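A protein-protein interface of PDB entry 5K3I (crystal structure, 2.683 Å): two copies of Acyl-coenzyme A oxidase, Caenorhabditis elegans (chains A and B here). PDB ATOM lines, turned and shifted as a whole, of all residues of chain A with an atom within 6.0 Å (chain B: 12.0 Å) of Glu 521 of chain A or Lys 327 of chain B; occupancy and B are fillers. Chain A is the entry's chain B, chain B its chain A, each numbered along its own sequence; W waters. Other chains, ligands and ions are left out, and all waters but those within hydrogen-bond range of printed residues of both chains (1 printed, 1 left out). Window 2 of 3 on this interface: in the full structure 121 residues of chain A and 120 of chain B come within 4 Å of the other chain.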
ATOM      1  N   ARG A 446      17.478   1.356   9.220  1.00  0.00           N
ATOM      2  CA  ARG A 446      16.952   2.325   8.254  1.00  0.00           C
ATOM      3  C   ARG A 446      15.428   2.392   8.327  1.00  0.00           C
ATOM      4  O   ARG A 446      14.837   3.479   8.354  1.00  0.00           O
ATOM      5  CB  ARG A 446      17.428   1.988   6.835  1.00  0.00           C
ATOM      6  CG  ARG A 446      18.924   2.141   6.662  1.00  0.00           C
ATOM      7  CD  ARG A 446      19.348   2.353   5.232  1.00  0.00           C
ATOM      8  NE  ARG A 446      20.643   3.031   5.196  1.00  0.00           N
ATOM      9  CZ  ARG A 446      20.798   4.352   5.233  1.00  0.00           C
ATOM     10  NH1 ARG A 446      19.741   5.147   5.298  1.00  0.00           N
ATOM     11  NH2 ARG A 446      22.013   4.879   5.204  1.00  0.00           N
ATOM     12  N   PHE A 510      21.021  10.818  15.249  1.00  0.00           N
ATOM     13  CA  PHE A 510      21.286  10.879  13.816  1.00  0.00           C
ATOM     14  C   PHE A 510      20.742  12.171  13.207  1.00  0.00           C
ATOM     15  O   PHE A 510      21.467  12.898  12.515  1.00  0.00           O
ATOM     16  CB  PHE A 510      20.686   9.638  13.150  1.00  0.00           C
ATOM     17  CG  PHE A 510      20.680   9.675  11.650  1.00  0.00           C
ATOM     18  CD1 PHE A 510      21.857   9.816  10.932  1.00  0.00           C
ATOM     19  CD2 PHE A 510      19.497   9.474  10.961  1.00  0.00           C
ATOM     20  CE1 PHE A 510      21.845   9.813   9.546  1.00  0.00           C
ATOM     21  CE2 PHE A 510      19.475   9.466   9.585  1.00  0.00           C
ATOM     22  CZ  PHE A 510      20.650   9.635   8.870  1.00  0.00           C
ATOM     23  N   LYS A 519      27.191  15.512   6.970  1.00  0.00           N
ATOM     24  CA  LYS A 519      26.593  14.791   5.849  1.00  0.00           C
ATOM     25  C   LYS A 519      25.802  13.583   6.341  1.00  0.00           C
ATOM     26  O   LYS A 519      26.137  12.963   7.352  1.00  0.00           O
ATOM     27  CB  LYS A 519      27.676  14.325   4.863  1.00  0.00           C
ATOM     28  CG  LYS A 519      28.579  15.422   4.298  1.00  0.00           C
ATOM     29  CD  LYS A 519      28.953  15.147   2.840  1.00  0.00           C
ATOM     30  CE  LYS A 519      27.720  15.024   1.961  1.00  0.00           C
ATOM     31  NZ  LYS A 519      28.010  15.378   0.542  1.00  0.00           N
ATOM     32  N   ARG A 520      24.734  13.261   5.602  1.00  0.00           N
ATOM     33  CA  ARG A 520      23.843  12.162   5.962  1.00  0.00           C
ATOM     34  C   ARG A 520      24.612  10.893   6.312  1.00  0.00           C
ATOM     35  O   ARG A 520      24.361  10.251   7.339  1.00  0.00           O
ATOM     36  CB  ARG A 520      22.868  11.893   4.815  1.00  0.00           C
ATOM     37  CG  ARG A 520      22.219  10.529   4.855  1.00  0.00           C
ATOM     38  CD  ARG A 520      21.001  10.474   3.960  1.00  0.00           C
ATOM     39  NE  ARG A 520      19.782  10.226   4.729  1.00  0.00           N
ATOM     40  CZ  ARG A 520      18.959  11.181   5.157  1.00  0.00           C
ATOM     41  NH1 ARG A 520      19.226  12.450   4.889  1.00  0.00           N
ATOM     42  NH2 ARG A 520      17.870  10.871   5.847  1.00  0.00           N
ATOM     43  N   GLU A 521      25.573  10.531   5.466  1.00  0.00           N
ATOM     44  CA  GLU A 521      26.206   9.225   5.575  1.00  0.00           C
ATOM     45  C   GLU A 521      27.268   9.194   6.665  1.00  0.00           C
ATOM     46  O   GLU A 521      27.500   8.140   7.266  1.00  0.00           O
ATOM     47  CB  GLU A 521      26.799   8.808   4.222  1.00  0.00           C
ATOM     48  CG  GLU A 521      25.885   9.089   3.019  1.00  0.00           C
ATOM     49  CD  GLU A 521      26.100  10.460   2.390  1.00  0.00           C
ATOM     50  OE1 GLU A 521      26.666  11.357   3.058  1.00  0.00           O
ATOM     51  OE2 GLU A 521      25.706  10.640   1.213  1.00  0.00           O
ATOM     52  N   ILE A 522      27.923  10.321   6.932  1.00  0.00           N
ATOM     53  CA  ILE A 522      28.863  10.389   8.049  1.00  0.00           C
ATOM     54  C   ILE A 522      28.122  10.421   9.384  1.00  0.00           C
ATOM     55  O   ILE A 522      28.544   9.788  10.358  1.00  0.00           O
ATOM     56  CB  ILE A 522      29.789  11.608   7.885  1.00  0.00           C
ATOM     57  CG1 ILE A 522      30.834  11.336   6.804  1.00  0.00           C
ATOM     58  CG2 ILE A 522      30.459  11.950   9.207  1.00  0.00           C
ATOM     59  CD1 ILE A 522      31.458  12.607   6.265  1.00  0.00           C
ATOM     60  N   ALA A 523      27.006  11.149   9.452  1.00  0.00           N
ATOM     61  CA  ALA A 523      26.154  11.093  10.637  1.00  0.00           C
ATOM     62  C   ALA A 523      25.617   9.683  10.855  1.00  0.00           C
ATOM     63  O   ALA A 523      25.486   9.227  11.998  1.00  0.00           O
ATOM     64  CB  ALA A 523      25.003  12.086  10.508  1.00  0.00           C
ATOM     65  N   TRP A 524      25.263   8.992   9.771  1.00  0.00           N
ATOM     66  CA  TRP A 524      24.827   7.605   9.886  1.00  0.00           C
ATOM     67  C   TRP A 524      25.918   6.736  10.497  1.00  0.00           C
ATOM     68  O   TRP A 524      25.672   5.988  11.451  1.00  0.00           O
ATOM     69  CB  TRP A 524      24.415   7.069   8.521  1.00  0.00           C
ATOM     70  CG  TRP A 524      23.927   5.681   8.598  1.00  0.00           C
ATOM     71  CD1 TRP A 524      24.641   4.540   8.365  1.00  0.00           C
ATOM     72  CD2 TRP A 524      22.617   5.269   8.976  1.00  0.00           C
ATOM     73  NE1 TRP A 524      23.841   3.440   8.549  1.00  0.00           N
ATOM     74  CE2 TRP A 524      22.593   3.862   8.928  1.00  0.00           C
ATOM     75  CE3 TRP A 524      21.453   5.954   9.341  1.00  0.00           C
ATOM     76  CZ2 TRP A 524      21.453   3.129   9.231  1.00  0.00           C
ATOM     77  CZ3 TRP A 524      20.320   5.220   9.639  1.00  0.00           C
ATOM     78  CH2 TRP A 524      20.327   3.822   9.582  1.00  0.00           C
ATOM     79  N   ASN A 525      27.124   6.781   9.921  1.00  0.00           N
ATOM     80  CA  ASN A 525      28.242   5.988  10.435  1.00  0.00           C
ATOM     81  C   ASN A 525      28.506   6.285  11.908  1.00  0.00           C
ATOM     82  O   ASN A 525      28.693   5.371  12.718  1.00  0.00           O
ATOM     83  CB  ASN A 525      29.502   6.251   9.604  1.00  0.00           C
ATOM     84  CG  ASN A 525      30.571   5.211   9.822  1.00  0.00           C
ATOM     85  OD1 ASN A 525      30.280   4.052  10.104  1.00  0.00           O
ATOM     86  ND2 ASN A 525      31.827   5.634   9.729  1.00  0.00           N
ATOM     87  N   LYS A 526      28.535   7.569  12.269  1.00  0.00           N
ATOM     88  CA  LYS A 526      28.762   7.961  13.657  1.00  0.00           C
ATOM     89  C   LYS A 526      27.671   7.480  14.610  1.00  0.00           C
ATOM     90  O   LYS A 526      27.909   7.427  15.823  1.00  0.00           O
ATOM     91  CB  LYS A 526      28.905   9.470  13.760  1.00  0.00           C
ATOM     92  CG  LYS A 526      30.229   9.951  13.231  1.00  0.00           C
ATOM     93  CD  LYS A 526      30.365  11.450  13.263  1.00  0.00           C
ATOM     94  CE  LYS A 526      31.820  11.814  13.056  1.00  0.00           C
ATOM     95  NZ  LYS A 526      32.053  13.270  12.909  1.00  0.00           N
ATOM     96  N   GLN B 322      34.517  -2.309   0.963  1.00  0.00           N
ATOM     97  CA  GLN B 322      33.148  -2.794   0.807  1.00  0.00           C
ATOM     98  C   GLN B 322      32.116  -1.725   1.148  1.00  0.00           C
ATOM     99  O   GLN B 322      31.940  -1.376   2.320  1.00  0.00           O
ATOM    100  CB  GLN B 322      32.923  -4.033   1.679  1.00  0.00           C
ATOM    101  CG  GLN B 322      31.765  -4.936   1.264  1.00  0.00           C
ATOM    102  CD  GLN B 322      31.948  -5.608  -0.098  1.00  0.00           C
ATOM    103  OE1 GLN B 322      30.988  -6.127  -0.671  1.00  0.00           O
ATOM    104  NE2 GLN B 322      33.172  -5.594  -0.621  1.00  0.00           N
ATOM    105  N   GLY B 323      31.434  -1.203   0.138  1.00  0.00           N
ATOM    106  CA  GLY B 323      30.400  -0.217   0.348  1.00  0.00           C
ATOM    107  C   GLY B 323      30.936   1.202   0.343  1.00  0.00           C
ATOM    108  O   GLY B 323      32.130   1.457   0.504  1.00  0.00           O
ATOM    109  N   GLN B 324      30.008   2.138   0.213  1.00  0.00           N
ATOM    110  CA  GLN B 324      30.303   3.559   0.211  1.00  0.00           C
ATOM    111  C   GLN B 324      29.740   4.229   1.452  1.00  0.00           C
ATOM    112  O   GLN B 324      28.665   3.873   1.936  1.00  0.00           O
ATOM    113  CB  GLN B 324      29.703   4.216  -1.029  1.00  0.00           C
ATOM    114  CG  GLN B 324      30.165   3.609  -2.313  1.00  0.00           C
ATOM    115  CD  GLN B 324      29.558   4.309  -3.501  1.00  0.00           C
ATOM    116  OE1 GLN B 324      28.534   3.878  -4.023  1.00  0.00           O
ATOM    117  NE2 GLN B 324      30.193   5.393  -3.947  1.00  0.00           N
ATOM    118  N   ILE B 325      30.475   5.212   1.954  1.00  0.00           N
ATOM    119  CA  ILE B 325      29.928   6.136   2.933  1.00  0.00           C
ATOM    120  C   ILE B 325      29.412   7.315   2.119  1.00  0.00           C
ATOM    121  O   ILE B 325      28.212   7.409   1.834  1.00  0.00           O
ATOM    122  CB  ILE B 325      30.975   6.526   3.992  1.00  0.00           C
ATOM    123  CG1 ILE B 325      31.357   5.286   4.807  1.00  0.00           C
ATOM    124  CG2 ILE B 325      30.447   7.615   4.911  1.00  0.00           C
ATOM    125  CD1 ILE B 325      32.310   5.544   5.948  1.00  0.00           C
ATOM    126  N   ASP B 326      30.315   8.197   1.701  1.00  0.00           N
ATOM    127  CA  ASP B 326      29.939   9.240   0.762  1.00  0.00           C
ATOM    128  C   ASP B 326      29.685   8.598  -0.603  1.00  0.00           C
ATOM    129  O   ASP B 326      30.506   7.817  -1.096  1.00  0.00           O
ATOM    130  CB  ASP B 326      31.041  10.295   0.689  1.00  0.00           C
ATOM    131  CG  ASP B 326      30.623  11.534  -0.073  1.00  0.00           C
ATOM    132  OD1 ASP B 326      30.238  11.418  -1.257  1.00  0.00           O
ATOM    133  OD2 ASP B 326      30.671  12.635   0.520  1.00  0.00           O
ATOM    134  N   LYS B 327      28.547   8.937  -1.217  1.00  0.00           N
ATOM    135  CA  LYS B 327      28.138   8.322  -2.476  1.00  0.00           C
ATOM    136  C   LYS B 327      29.024   8.701  -3.654  1.00  0.00           C
ATOM    137  O   LYS B 327      29.017   7.995  -4.670  1.00  0.00           O
ATOM    138  CB  LYS B 327      26.703   8.723  -2.816  1.00  0.00           C
ATOM    139  CG  LYS B 327      25.657   8.354  -1.790  1.00  0.00           C
ATOM    140  CD  LYS B 327      25.155   6.936  -1.976  1.00  0.00           C
ATOM    141  CE  LYS B 327      23.843   6.746  -1.230  1.00  0.00           C
ATOM    142  NZ  LYS B 327      24.018   6.940   0.236  1.00  0.00           N
ATOM    143  N   ASN B 328      29.744   9.817  -3.575  1.00  0.00           N
ATOM    144  CA  ASN B 328      30.663  10.223  -4.635  1.00  0.00           C
ATOM    145  C   ASN B 328      32.110   9.795  -4.405  1.00  0.00           C
ATOM    146  O   ASN B 328      32.960  10.044  -5.268  1.00  0.00           O
ATOM    147  CB  ASN B 328      30.562  11.739  -4.817  1.00  0.00           C
ATOM    148  CG  ASN B 328      29.148  12.183  -5.154  1.00  0.00           C
ATOM    149  OD1 ASN B 328      28.515  11.643  -6.069  1.00  0.00           O
ATOM    150  ND2 ASN B 328      28.638  13.151  -4.402  1.00  0.00           N
ATOM    151  N   GLU B 329      32.413   9.164  -3.286  1.00  0.00           N
ATOM    152  CA  GLU B 329      33.758   8.653  -3.059  1.00  0.00           C
ATOM    153  C   GLU B 329      33.786   7.143  -3.259  1.00  0.00           C
ATOM    154  O   GLU B 329      32.750   6.479  -3.178  1.00  0.00           O
ATOM    155  CB  GLU B 329      34.227   9.026  -1.651  1.00  0.00           C
ATOM    156  CG  GLU B 329      34.207  10.529  -1.413  1.00  0.00           C
ATOM    157  CD  GLU B 329      34.898  10.948  -0.135  1.00  0.00           C
ATOM    158  OE1 GLU B 329      35.057  10.109   0.779  1.00  0.00           O
ATOM    159  OE2 GLU B 329      35.290  12.130  -0.050  1.00  0.00           O
ATOM    160  N   PRO B 330      34.951   6.555  -3.528  1.00  0.00           N
ATOM    161  CA  PRO B 330      35.001   5.108  -3.789  1.00  0.00           C
ATOM    162  C   PRO B 330      34.651   4.306  -2.540  1.00  0.00           C
ATOM    163  O   PRO B 330      34.482   4.841  -1.440  1.00  0.00           O
ATOM    164  CB  PRO B 330      36.452   4.847  -4.224  1.00  0.00           C
ATOM    165  CG  PRO B 330      37.183   6.133  -4.104  1.00  0.00           C
ATOM    166  CD  PRO B 330      36.254   7.225  -3.695  1.00  0.00           C
ATOM    167  N   GLU B 331      34.529   2.991  -2.738  1.00  0.00           N
ATOM    168  CA  GLU B 331      34.304   2.066  -1.630  1.00  0.00           C
ATOM    169  C   GLU B 331      35.343   2.246  -0.528  1.00  0.00           C
ATOM    170  O   GLU B 331      36.544   2.345  -0.792  1.00  0.00           O
ATOM    171  CB  GLU B 331      34.316   0.624  -2.149  1.00  0.00           C
ATOM    172  CG  GLU B 331      33.028   0.215  -2.848  1.00  0.00           C
ATOM    173  CD  GLU B 331      32.995  -1.253  -3.231  1.00  0.00           C
ATOM    174  OE1 GLU B 331      33.854  -1.681  -4.029  1.00  0.00           O
ATOM    175  OE2 GLU B 331      32.107  -1.981  -2.744  1.00  0.00           O
ATOM    176  N   VAL B 332      34.865   2.280   0.723  1.00  0.00           N
ATOM    177  CA  VAL B 332      35.718   2.500   1.888  1.00  0.00           C
ATOM    178  C   VAL B 332      36.263   1.179   2.418  1.00  0.00           C
ATOM    179  O   VAL B 332      35.678   0.106   2.226  1.00  0.00           O
ATOM    180  CB  VAL B 332      34.950   3.256   2.998  1.00  0.00           C
ATOM    181  CG1 VAL B 332      34.401   4.561   2.472  1.00  0.00           C
ATOM    182  CG2 VAL B 332      33.850   2.390   3.597  1.00  0.00           C
ATOM    183  N   LYS B 333      37.434   1.265   3.052  1.00  0.00           N
ATOM    184  CA  LYS B 333      37.905   0.208   3.937  1.00  0.00           C
ATOM    185  C   LYS B 333      36.804  -0.116   4.935  1.00  0.00           C
ATOM    186  O   LYS B 333      36.168   0.792   5.471  1.00  0.00           O
ATOM    187  CB  LYS B 333      39.153   0.676   4.689  1.00  0.00           C
ATOM    188  CG  LYS B 333      40.391   0.840   3.844  1.00  0.00           C
ATOM    189  CD  LYS B 333      41.526   1.417   4.668  1.00  0.00           C
ATOM    190  CE  LYS B 333      42.682   1.839   3.770  1.00  0.00           C
ATOM    191  NZ  LYS B 333      43.816   2.443   4.528  1.00  0.00           N
ATOM    192  N   GLU B 336      36.552   1.384   8.450  1.00  0.00           N
ATOM    193  CA  GLU B 336      36.107   2.766   8.596  1.00  0.00           C
ATOM    194  C   GLU B 336      34.757   2.867   9.302  1.00  0.00           C
ATOM    195  O   GLU B 336      34.474   3.856   9.979  1.00  0.00           O
ATOM    196  CB  GLU B 336      36.035   3.451   7.229  1.00  0.00           C
ATOM    197  CG  GLU B 336      36.786   4.771   7.156  1.00  0.00           C
ATOM    198  CD  GLU B 336      38.038   4.683   6.307  1.00  0.00           C
ATOM    199  OE1 GLU B 336      38.979   5.466   6.550  1.00  0.00           O
ATOM    200  OE2 GLU B 336      38.082   3.829   5.396  1.00  0.00           O
ATOM    201  N   TYR B 337      33.928   1.841   9.142  1.00  0.00           N
ATOM    202  CA  TYR B 337      32.608   1.822   9.762  1.00  0.00           C
ATOM    203  C   TYR B 337      32.706   1.710  11.279  1.00  0.00           C
ATOM    204  O   TYR B 337      33.494   0.922  11.800  1.00  0.00           O
ATOM    205  CB  TYR B 337      31.779   0.657   9.217  1.00  0.00           C
ATOM    206  CG  TYR B 337      31.568   0.687   7.720  1.00  0.00           C
ATOM    207  CD1 TYR B 337      30.815   1.689   7.125  1.00  0.00           C
ATOM    208  CD2 TYR B 337      32.119  -0.292   6.904  1.00  0.00           C
ATOM    209  CE1 TYR B 337      30.618   1.717   5.758  1.00  0.00           C
ATOM    210  CE2 TYR B 337      31.927  -0.272   5.536  1.00  0.00           C
ATOM    211  CZ  TYR B 337      31.176   0.734   4.969  1.00  0.00           C
ATOM    212  OH  TYR B 337      30.983   0.757   3.608  1.00  0.00           O
ATOM    213  N   GLN B 338      31.901   2.497  11.986  1.00  0.00           N
ATOM    214  CA  GLN B 338      31.901   2.461  13.446  1.00  0.00           C
ATOM    215  C   GLN B 338      31.532   1.078  13.981  1.00  0.00           C
ATOM    216  O   GLN B 338      32.022   0.681  15.041  1.00  0.00           O
ATOM    217  CB  GLN B 338      30.946   3.515  13.986  1.00  0.00           C
ATOM    218  CG  GLN B 338      31.176   3.925  15.417  1.00  0.00           C
ATOM    219  CD  GLN B 338      29.999   4.697  15.959  1.00  0.00           C
ATOM    220  OE1 GLN B 338      28.877   4.211  15.923  1.00  0.00           O
ATOM    221  NE2 GLN B 338      30.247   5.895  16.480  1.00  0.00           N
ATOM    222  N   THR B 339      30.659   0.333  13.284  1.00  0.00           N
ATOM    223  CA  THR B 339      30.350  -1.028  13.728  1.00  0.00           C
ATOM    224  C   THR B 339      31.573  -1.919  13.672  1.00  0.00           C
ATOM    225  O   THR B 339      31.723  -2.822  14.500  1.00  0.00           O
ATOM    226  CB  THR B 339      29.255  -1.693  12.883  1.00  0.00           C
ATOM    227  OG1 THR B 339      29.695  -1.797  11.517  1.00  0.00           O
ATOM    228  CG2 THR B 339      27.906  -1.019  13.024  1.00  0.00           C
HETATM  229  O   HOH W   1      30.149  14.507  -1.826  1.00  0.00           O
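Water W1 lies within hydrogen-bond range of OD2 of Asp 326 of chain B, ND2 of Asn 328 of chain B and NZ of Lys 519 of chain A.
No position is printed for both chains. Of the 8 pairs that touch across the chains among the printed residues, none has its exchanged pair printed and touching as well.
Glu 521 of chain A touches just these residues of chain B: Ile 325 and Lys 327. Of the printed residues of chain A, Lys 327 of chain B touches Glu 521 (3.8 Å). Lys 519 of chain A touches one residue of chain B. No residue of chain B comes within 4 Å of Ile 522 of chain A. No residue of chain B comes within 4 Å of Ala 523 of chain A. Of the printed residues of chain B, Asn 525 of chain A touches Ile 325 (3.8 Å), Glu 336 (3.2 Å), Tyr 337 (3.2 Å) and Gln 338 (2.9 Å). Of the printed residues of chain A, Gln 338 of chain B touches Asn 525 (2.9 Å) and Lys 526 (2.9 Å). Of the printed residues of chain A, Tyr 337 of chain B touches Asn 525. Of the printed residues of chain B, Lys 526 of chain A touches Gln 338 (2.9 Å). Printed residues of chain A within 4 Å of Glu 336 of chain B: Asn 525 (3.2 Å). Printed residues of chain A within 4 Å of Asp 326 of chain B: Lys 519. The nearest residue of chain A that does not touch Lys 327 of chain B is Arg 446 of chain A (5.7 Å). The nearest printed residue of chain A that does not touch Ile 325 of chain B is Ile 522 of chain A (4.2 Å).
Of the 16 printed residues of chain B, 6 touch a printed residue of chain A. Printed residues of chain B that touch a printed residue of chain A: Ile 325, Asp 326, Lys 327, Glu 336, Tyr 337 and Gln 338. Hydrophobic or aromatic side chains of chain B that line the printed part of chain A: Ile 325 and Tyr 337. Of the 10 printed residues of chain A, 4 touch a printed residue of chain B. Among the printed residues, 8 pairs touch across the chains.
Among the printed residues, pairs that only touch across the chains: Glu 521 of chain A with Ile 325 of chain B (3.1 Å), Glu 521 of chain A with Lys 327 of chain B (3.8 Å), Asn 525 of chain A with Ile 325 of chain B (3.8 Å) and Asn 525 of chain A with Tyr 337 of chain B (3.2 Å).
The backbone carbonyl oxygen (O) of Gln 322 of chain B lies within hydrogen-bond range of the side-chain hydroxyl (OH) of Tyr 337 of chain B, 2.7 Å away. The backbone carbonyl oxygen (O) of Gly 323 of chain B lies close to the side-chain hydroxyl (OH) of Tyr 337 of chain B (3.4 Å). The backbone carbonyl oxygen of Lys 327 of chain B is in hydrogen-bond range of the side-chain amide nitrogen of Gln 324 of chain B (2.9 Å). The side-chain carboxylate (OD1) of Asp 326 of chain B sits at hydrogen-bond distance from the backbone NH (N) of Asn 328 of chain B (2.9 Å).
OD2 of Asp 326 of chain B is in salt-bridge range of NZ of Lys 519 of chain A, 3.8 Å away. ND2 of Asn 525 of chain A is in hydrogen-bond range of O of Glu 336 of chain B. The side-chain amide oxygen (OD1) of Asn 525 of chain A sits at hydrogen-bond distance from the backbone NH (N) of Gln 338 of chain B (2.9 Å). NE2 of Gln 338 of chain B lies within hydrogen-bond range of O of Lys 526 of chain A.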
